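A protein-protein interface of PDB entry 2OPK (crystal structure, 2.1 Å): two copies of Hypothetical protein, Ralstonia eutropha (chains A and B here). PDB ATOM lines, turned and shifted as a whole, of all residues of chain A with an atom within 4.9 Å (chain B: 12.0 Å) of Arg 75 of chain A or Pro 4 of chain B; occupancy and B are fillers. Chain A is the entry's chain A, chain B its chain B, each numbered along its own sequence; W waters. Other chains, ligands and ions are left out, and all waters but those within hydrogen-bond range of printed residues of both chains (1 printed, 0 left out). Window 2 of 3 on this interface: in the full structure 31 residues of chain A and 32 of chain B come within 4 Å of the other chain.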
ATOM      1  N   ALA A  64      31.355 -13.579  25.779  1.00  0.00           N
ATOM      2  CA  ALA A  64      32.190 -13.780  24.609  1.00  0.00           C
ATOM      3  C   ALA A  64      31.459 -13.429  23.348  1.00  0.00           C
ATOM      4  O   ALA A  64      30.227 -13.286  23.333  1.00  0.00           O
ATOM      5  CB  ALA A  64      32.610 -15.214  24.509  1.00  0.00           C
ATOM      6  N   GLY A  65      32.236 -13.303  22.276  1.00  0.00           N
ATOM      7  CA  GLY A  65      31.658 -13.205  20.949  1.00  0.00           C
ATOM      8  C   GLY A  65      32.145 -14.339  20.096  1.00  0.00           C
ATOM      9  O   GLY A  65      33.335 -14.609  20.019  1.00  0.00           O
ATOM     10  N   ILE A  66      31.215 -15.013  19.450  1.00  0.00           N
ATOM     11  CA  ILE A  66      31.549 -16.040  18.499  1.00  0.00           C
ATOM     12  C   ILE A  66      31.049 -15.596  17.120  1.00  0.00           C
ATOM     13  O   ILE A  66      29.950 -15.084  16.970  1.00  0.00           O
ATOM     14  CB  ILE A  66      30.939 -17.394  18.873  1.00  0.00           C
ATOM     15  CG1 ILE A  66      31.593 -17.874  20.178  1.00  0.00           C
ATOM     16  CG2 ILE A  66      31.112 -18.395  17.738  1.00  0.00           C
ATOM     17  CD1 ILE A  66      31.414 -19.334  20.501  1.00  0.00           C
ATOM     18  N   GLU A  67      31.865 -15.867  16.122  1.00  0.00           N
ATOM     19  CA  GLU A  67      31.596 -15.492  14.766  1.00  0.00           C
ATOM     20  C   GLU A  67      31.640 -16.769  13.948  1.00  0.00           C
ATOM     21  O   GLU A  67      32.652 -17.478  13.931  1.00  0.00           O
ATOM     22  CB  GLU A  67      32.693 -14.510  14.369  1.00  0.00           C
ATOM     23  CG  GLU A  67      32.524 -13.832  13.048  1.00  0.00           C
ATOM     24  CD  GLU A  67      33.787 -13.087  12.629  1.00  0.00           C
ATOM     25  OE1 GLU A  67      34.638 -12.776  13.521  1.00  0.00           O
ATOM     26  OE2 GLU A  67      33.920 -12.861  11.398  1.00  0.00           O
ATOM     27  N   CYS A  68      30.497 -17.125  13.358  1.00  0.00           N
ATOM     28  CA  CYS A  68      30.411 -18.246  12.414  1.00  0.00           C
ATOM     29  C   CYS A  68      30.682 -17.680  11.043  1.00  0.00           C
ATOM     30  O   CYS A  68      30.365 -16.510  10.785  1.00  0.00           O
ATOM     31  CB  CYS A  68      29.047 -18.897  12.455  1.00  0.00           C
ATOM     32  SG  CYS A  68      28.809 -19.779  13.969  1.00  0.00           S
ATOM     33  N   ASP A  71      28.792 -14.732   9.168  1.00  0.00           N
ATOM     34  CA  ASP A  71      28.226 -13.755  10.092  1.00  0.00           C
ATOM     35  C   ASP A  71      28.739 -12.371   9.788  1.00  0.00           C
ATOM     36  O   ASP A  71      29.905 -12.199   9.501  1.00  0.00           O
ATOM     37  CB  ASP A  71      28.622 -14.038  11.543  1.00  0.00           C
ATOM     38  CG  ASP A  71      27.922 -15.220  12.141  1.00  0.00           C
ATOM     39  OD1 ASP A  71      27.093 -15.859  11.461  1.00  0.00           O
ATOM     40  OD2 ASP A  71      28.233 -15.506  13.316  1.00  0.00           O
ATOM     41  N   ALA A  73      28.514  -9.929  12.111  1.00  0.00           N
ATOM     42  CA  ALA A  73      29.055  -9.497  13.396  1.00  0.00           C
ATOM     43  C   ALA A  73      29.147 -10.689  14.348  1.00  0.00           C
ATOM     44  O   ALA A  73      28.468 -11.707  14.140  1.00  0.00           O
ATOM     45  CB  ALA A  73      28.181  -8.443  14.002  1.00  0.00           C
ATOM     46  N   PRO A  74      30.008 -10.581  15.379  1.00  0.00           N
ATOM     47  CA  PRO A  74      30.043 -11.647  16.359  1.00  0.00           C
ATOM     48  C   PRO A  74      28.727 -11.778  17.125  1.00  0.00           C
ATOM     49  O   PRO A  74      28.068 -10.791  17.410  1.00  0.00           O
ATOM     50  CB  PRO A  74      31.181 -11.218  17.301  1.00  0.00           C
ATOM     51  CG  PRO A  74      32.003 -10.255  16.525  1.00  0.00           C
ATOM     52  CD  PRO A  74      31.033  -9.549  15.652  1.00  0.00           C
ATOM     53  N   ARG A  75      28.358 -13.008  17.423  1.00  0.00           N
ATOM     54  CA  ARG A  75      27.232 -13.326  18.266  1.00  0.00           C
ATOM     55  C   ARG A  75      27.666 -13.174  19.725  1.00  0.00           C
ATOM     56  O   ARG A  75      28.510 -13.912  20.213  1.00  0.00           O
ATOM     57  CB  ARG A  75      26.804 -14.772  18.038  1.00  0.00           C
ATOM     58  CG  ARG A  75      26.399 -15.110  16.603  1.00  0.00           C
ATOM     59  CD  ARG A  75      26.612 -16.568  16.298  1.00  0.00           C
ATOM     60  NE  ARG A  75      26.324 -16.829  14.893  1.00  0.00           N
ATOM     61  CZ  ARG A  75      25.213 -17.392  14.400  1.00  0.00           C
ATOM     62  NH1 ARG A  75      24.240 -17.867  15.181  1.00  0.00           N
ATOM     63  NH2 ARG A  75      25.098 -17.516  13.082  1.00  0.00           N
ATOM     64  N   VAL A  76      27.072 -12.212  20.414  1.00  0.00           N
ATOM     65  CA  VAL A  76      27.368 -11.923  21.803  1.00  0.00           C
ATOM     66  C   VAL A  76      26.714 -12.982  22.716  1.00  0.00           C
ATOM     67  O   VAL A  76      25.517 -13.188  22.682  1.00  0.00           O
ATOM     68  CB  VAL A  76      26.869 -10.534  22.183  1.00  0.00           C
ATOM     69  CG1 VAL A  76      27.166 -10.253  23.659  1.00  0.00           C
ATOM     70  CG2 VAL A  76      27.513  -9.441  21.243  1.00  0.00           C
ATOM     71  N   MET A  77      27.522 -13.661  23.519  1.00  0.00           N
ATOM     72  CA  MET A  77      27.027 -14.718  24.404  1.00  0.00           C
ATOM     73  C   MET A  77      27.289 -14.348  25.851  1.00  0.00           C
ATOM     74  O   MET A  77      28.406 -13.979  26.208  1.00  0.00           O
ATOM     75  CB  MET A  77      27.673 -16.050  24.020  1.00  0.00           C
ATOM     76  CG  MET A  77      27.274 -16.497  22.571  1.00  0.00           C
ATOM     77  SD  MET A  77      28.150 -18.080  22.060  1.00  0.00           S
ATOM     78  CE  MET A  77      27.069 -19.325  23.148  1.00  0.00           C
ATOM     79  N   LEU A  83      25.003 -22.351  21.796  1.00  0.00           N
ATOM     80  CA  LEU A  83      25.125 -22.323  20.360  1.00  0.00           C
ATOM     81  C   LEU A  83      25.499 -23.722  19.931  1.00  0.00           C
ATOM     82  O   LEU A  83      26.412 -24.328  20.512  1.00  0.00           O
ATOM     83  CB  LEU A  83      26.244 -21.349  19.954  1.00  0.00           C
ATOM     84  CG  LEU A  83      26.609 -21.260  18.454  1.00  0.00           C
ATOM     85  CD1 LEU A  83      25.472 -20.747  17.642  1.00  0.00           C
ATOM     86  CD2 LEU A  83      27.853 -20.378  18.245  1.00  0.00           C
ATOM     87  N   HIS A  84      24.793 -24.227  18.919  1.00  0.00           N
ATOM     88  CA  HIS A  84      25.110 -25.504  18.297  1.00  0.00           C
ATOM     89  C   HIS A  84      25.810 -25.208  16.978  1.00  0.00           C
ATOM     90  O   HIS A  84      25.266 -24.510  16.112  1.00  0.00           O
ATOM     91  CB  HIS A  84      23.851 -26.324  18.074  1.00  0.00           C
ATOM     92  CG  HIS A  84      24.059 -27.549  17.237  1.00  0.00           C
ATOM     93  ND1 HIS A  84      23.263 -27.842  16.149  1.00  0.00           N
ATOM     94  CD2 HIS A  84      24.989 -28.529  17.299  1.00  0.00           C
ATOM     95  CE1 HIS A  84      23.680 -28.971  15.597  1.00  0.00           C
ATOM     96  NE2 HIS A  84      24.726 -29.407  16.272  1.00  0.00           N
ATOM     97  N   PRO A  86      27.229 -26.989  13.862  1.00  0.00           N
ATOM     98  CA  PRO A  86      27.272 -28.240  13.159  1.00  0.00           C
ATOM     99  C   PRO A  86      28.661 -28.576  12.613  1.00  0.00           C
ATOM    100  O   PRO A  86      29.439 -27.686  12.335  1.00  0.00           O
ATOM    101  CB  PRO A  86      26.301 -27.986  11.998  1.00  0.00           C
ATOM    102  CG  PRO A  86      25.408 -26.901  12.505  1.00  0.00           C
ATOM    103  CD  PRO A  86      26.341 -26.027  13.177  1.00  0.00           C
ATOM    104  N   CYS A  89      30.998 -26.510  10.077  1.00  0.00           N
ATOM    105  CA  CYS A  89      30.663 -25.092  10.124  1.00  0.00           C
ATOM    106  C   CYS A  89      31.858 -24.386  10.753  1.00  0.00           C
ATOM    107  O   CYS A  89      32.181 -24.640  11.883  1.00  0.00           O
ATOM    108  CB  CYS A  89      29.413 -24.851  10.983  1.00  0.00           C
ATOM    109  SG  CYS A  89      29.043 -23.070  11.236  1.00  0.00           S
ATOM    110  N   MET B   2      22.979 -28.016   9.070  1.00  0.00           N
ATOM    111  CA  MET B   2      23.757 -27.041   8.235  1.00  0.00           C
ATOM    112  C   MET B   2      23.924 -25.685   8.944  1.00  0.00           C
ATOM    113  O   MET B   2      25.058 -25.228   9.175  1.00  0.00           O
ATOM    114  CB  MET B   2      23.078 -26.826   6.867  1.00  0.00           C
ATOM    115  N   ASP B   3      22.799 -25.046   9.275  1.00  0.00           N
ATOM    116  CA  ASP B   3      22.821 -23.745   9.958  1.00  0.00           C
ATOM    117  C   ASP B   3      22.916 -23.921  11.505  1.00  0.00           C
ATOM    118  O   ASP B   3      22.360 -24.885  12.074  1.00  0.00           O
ATOM    119  CB  ASP B   3      21.600 -22.895   9.563  1.00  0.00           C
ATOM    120  N   PRO B   4      23.641 -23.005  12.181  1.00  0.00           N
ATOM    121  CA  PRO B   4      23.742 -23.041  13.634  1.00  0.00           C
ATOM    122  C   PRO B   4      22.467 -22.599  14.356  1.00  0.00           C
ATOM    123  O   PRO B   4      21.833 -21.627  13.934  1.00  0.00           O
ATOM    124  CB  PRO B   4      24.854 -22.036  13.924  1.00  0.00           C
ATOM    125  CG  PRO B   4      24.783 -21.074  12.804  1.00  0.00           C
ATOM    126  CD  PRO B   4      24.422 -21.892  11.609  1.00  0.00           C
ATOM    127  N   LYS B   5      22.097 -23.319  15.422  1.00  0.00           N
ATOM    128  CA  LYS B   5      20.991 -22.906  16.285  1.00  0.00           C
ATOM    129  C   LYS B   5      21.532 -22.364  17.614  1.00  0.00           C
ATOM    130  O   LYS B   5      22.644 -22.656  18.028  1.00  0.00           O
ATOM    131  CB  LYS B   5      19.943 -24.005  16.492  1.00  0.00           C
ATOM    132  CG  LYS B   5      20.396 -25.318  17.057  1.00  0.00           C
ATOM    133  N   HIS B   6      20.741 -21.528  18.259  1.00  0.00           N
ATOM    134  CA  HIS B   6      21.154 -20.913  19.498  1.00  0.00           C
ATOM    135  C   HIS B   6      19.956 -20.728  20.400  1.00  0.00           C
ATOM    136  O   HIS B   6      18.803 -20.832  19.956  1.00  0.00           O
ATOM    137  CB  HIS B   6      21.863 -19.592  19.219  1.00  0.00           C
ATOM    138  CG  HIS B   6      20.979 -18.539  18.641  1.00  0.00           C
ATOM    139  ND1 HIS B   6      20.419 -17.538  19.405  1.00  0.00           N
ATOM    140  CD2 HIS B   6      20.580 -18.312  17.368  1.00  0.00           C
ATOM    141  CE1 HIS B   6      19.705 -16.746  18.627  1.00  0.00           C
ATOM    142  NE2 HIS B   6      19.780 -17.198  17.390  1.00  0.00           N
ATOM    143  N   GLY B   7      20.234 -20.481  21.675  1.00  0.00           N
ATOM    144  CA  GLY B   7      19.191 -20.280  22.653  1.00  0.00           C
ATOM    145  C   GLY B   7      19.792 -19.768  23.942  1.00  0.00           C
ATOM    146  O   GLY B   7      20.999 -19.500  24.026  1.00  0.00           O
ATOM    147  N   ASN B   8      18.918 -19.589  24.921  1.00  0.00           N
ATOM    148  CA  ASN B   8      19.321 -19.236  26.254  1.00  0.00           C
ATOM    149  C   ASN B   8      18.588 -20.174  27.183  1.00  0.00           C
ATOM    150  O   ASN B   8      17.367 -20.340  27.061  1.00  0.00           O
ATOM    151  CB  ASN B   8      19.020 -17.780  26.590  1.00  0.00           C
ATOM    152  CG  ASN B   8      19.593 -17.378  27.930  1.00  0.00           C
ATOM    153  OD1 ASN B   8      19.021 -17.679  28.979  1.00  0.00           O
ATOM    154  ND2 ASN B   8      20.736 -16.711  27.906  1.00  0.00           N
ATOM    155  N   LEU B  25      17.727 -29.997  23.476  1.00  0.00           N
ATOM    156  CA  LEU B  25      18.481 -28.963  22.789  1.00  0.00           C
ATOM    157  C   LEU B  25      19.258 -29.543  21.612  1.00  0.00           C
ATOM    158  O   LEU B  25      19.412 -28.903  20.617  1.00  0.00           O
ATOM    159  CB  LEU B  25      19.459 -28.321  23.779  1.00  0.00           C
ATOM    160  CG  LEU B  25      18.879 -27.760  25.083  1.00  0.00           C
ATOM    161  CD1 LEU B  25      19.940 -27.127  25.934  1.00  0.00           C
ATOM    162  CD2 LEU B  25      17.806 -26.758  24.776  1.00  0.00           C
ATOM    163  N   LEU B  26      19.796 -30.742  21.753  1.00  0.00           N
ATOM    164  CA  LEU B  26      20.432 -31.423  20.643  1.00  0.00           C
ATOM    165  C   LEU B  26      20.174 -32.914  20.716  1.00  0.00           C
ATOM    166  O   LEU B  26      20.278 -33.505  21.797  1.00  0.00           O
ATOM    167  CB  LEU B  26      21.935 -31.132  20.658  1.00  0.00           C
ATOM    168  CG  LEU B  26      22.755 -31.689  19.485  1.00  0.00           C
ATOM    169  CD1 LEU B  26      22.345 -30.973  18.204  1.00  0.00           C
ATOM    170  CD2 LEU B  26      24.219 -31.458  19.749  1.00  0.00           C
ATOM    171  N   ARG B  28      21.297 -36.454  18.572  1.00  0.00           N
ATOM    172  CA  ARG B  28      22.146 -37.174  17.608  1.00  0.00           C
ATOM    173  C   ARG B  28      22.137 -38.640  18.029  1.00  0.00           C
ATOM    174  O   ARG B  28      21.754 -38.946  19.136  1.00  0.00           O
ATOM    175  CB  ARG B  28      23.578 -36.634  17.636  1.00  0.00           C
ATOM    176  CG  ARG B  28      23.739 -35.176  17.142  1.00  0.00           C
ATOM    177  CD  ARG B  28      23.599 -35.141  15.636  1.00  0.00           C
ATOM    178  NE  ARG B  28      23.629 -33.810  15.015  1.00  0.00           N
ATOM    179  CZ  ARG B  28      22.559 -33.046  14.767  1.00  0.00           C
ATOM    180  NH1 ARG B  28      21.325 -33.401  15.147  1.00  0.00           N
ATOM    181  NH2 ARG B  28      22.720 -31.884  14.144  1.00  0.00           N
HETATM  182  O   HOH W   1      21.703 -19.128  13.373  1.00  0.00           O
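The backbone NH (N) of His 84 of chain A is in hydrogen-bond range of the backbone carbonyl oxygen (O) of Lys 5 of chain B, 2.8 Å away.
N of Arg 75 of chain A is in hydrogen-bond range of O of Ile 66 of chain A (2.7 Å). NE of Arg 75 of chain A lies within salt-bridge range of OD2 of Asp 71 of chain A (2.8 Å).
Among the printed residues, pairs that only touch across the chains: Arg 75 of chain A with Pro 4 of chain B (3.6 Å), Leu 83 of chain A with Pro 4 of chain B (3.98 Å), Leu 83 of chain A with Lys 5 of chain B (3.4 Å), His 84 of chain A with Pro 4 of chain B (3.3 Å), His 84 of chain A with Leu 26 of chain B (3.4 Å), His 84 of chain A with Arg 28 of chain B (3.4 Å), Pro 86 of chain A with Met 2 of chain B (3.7 Å), Pro 86 of chain A with Asp 3 of chain B (3.7 Å) and Pro 86 of chain A with Pro 4 of chain B (3.98 Å).
Of chain B, only Pro 4 (3.6 Å) comes within 4 Å of Arg 75 of chain A. Printed residues of chain A within 4 Å of Pro 4 of chain B: Arg 75 (3.6 Å), Leu 83 (3.98 Å), His 84 (3.3 Å) and Pro 86 (3.98 Å). No residue of chain B comes within 4 Å of Gly 65 of chain A. No residue of chain B comes within 4 Å of Cys 68 of chain A. His 84 of chain A touches four residues of chain B. Of the printed residues of chain A, Leu 26 of chain B touches His 84. Printed residues of chain A within 4 Å of Arg 28 of chain B: His 84 (3.4 Å). Of the printed residues of chain A, Met 2 of chain B touches Pro 86. Asn 8 of chain B touches none of the printed residues of chain A.
Among the printed residues, no Asp or Glu carboxylate lies within 4 Å of a Lys or Arg side-chain nitrogen of the other chain.
No position is printed for both chains.
Water W1 lies within hydrogen-bond range of O of Pro 4 of chain B (2.6 Å) and NH1 of Arg 75 of chain A (3.4 Å).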
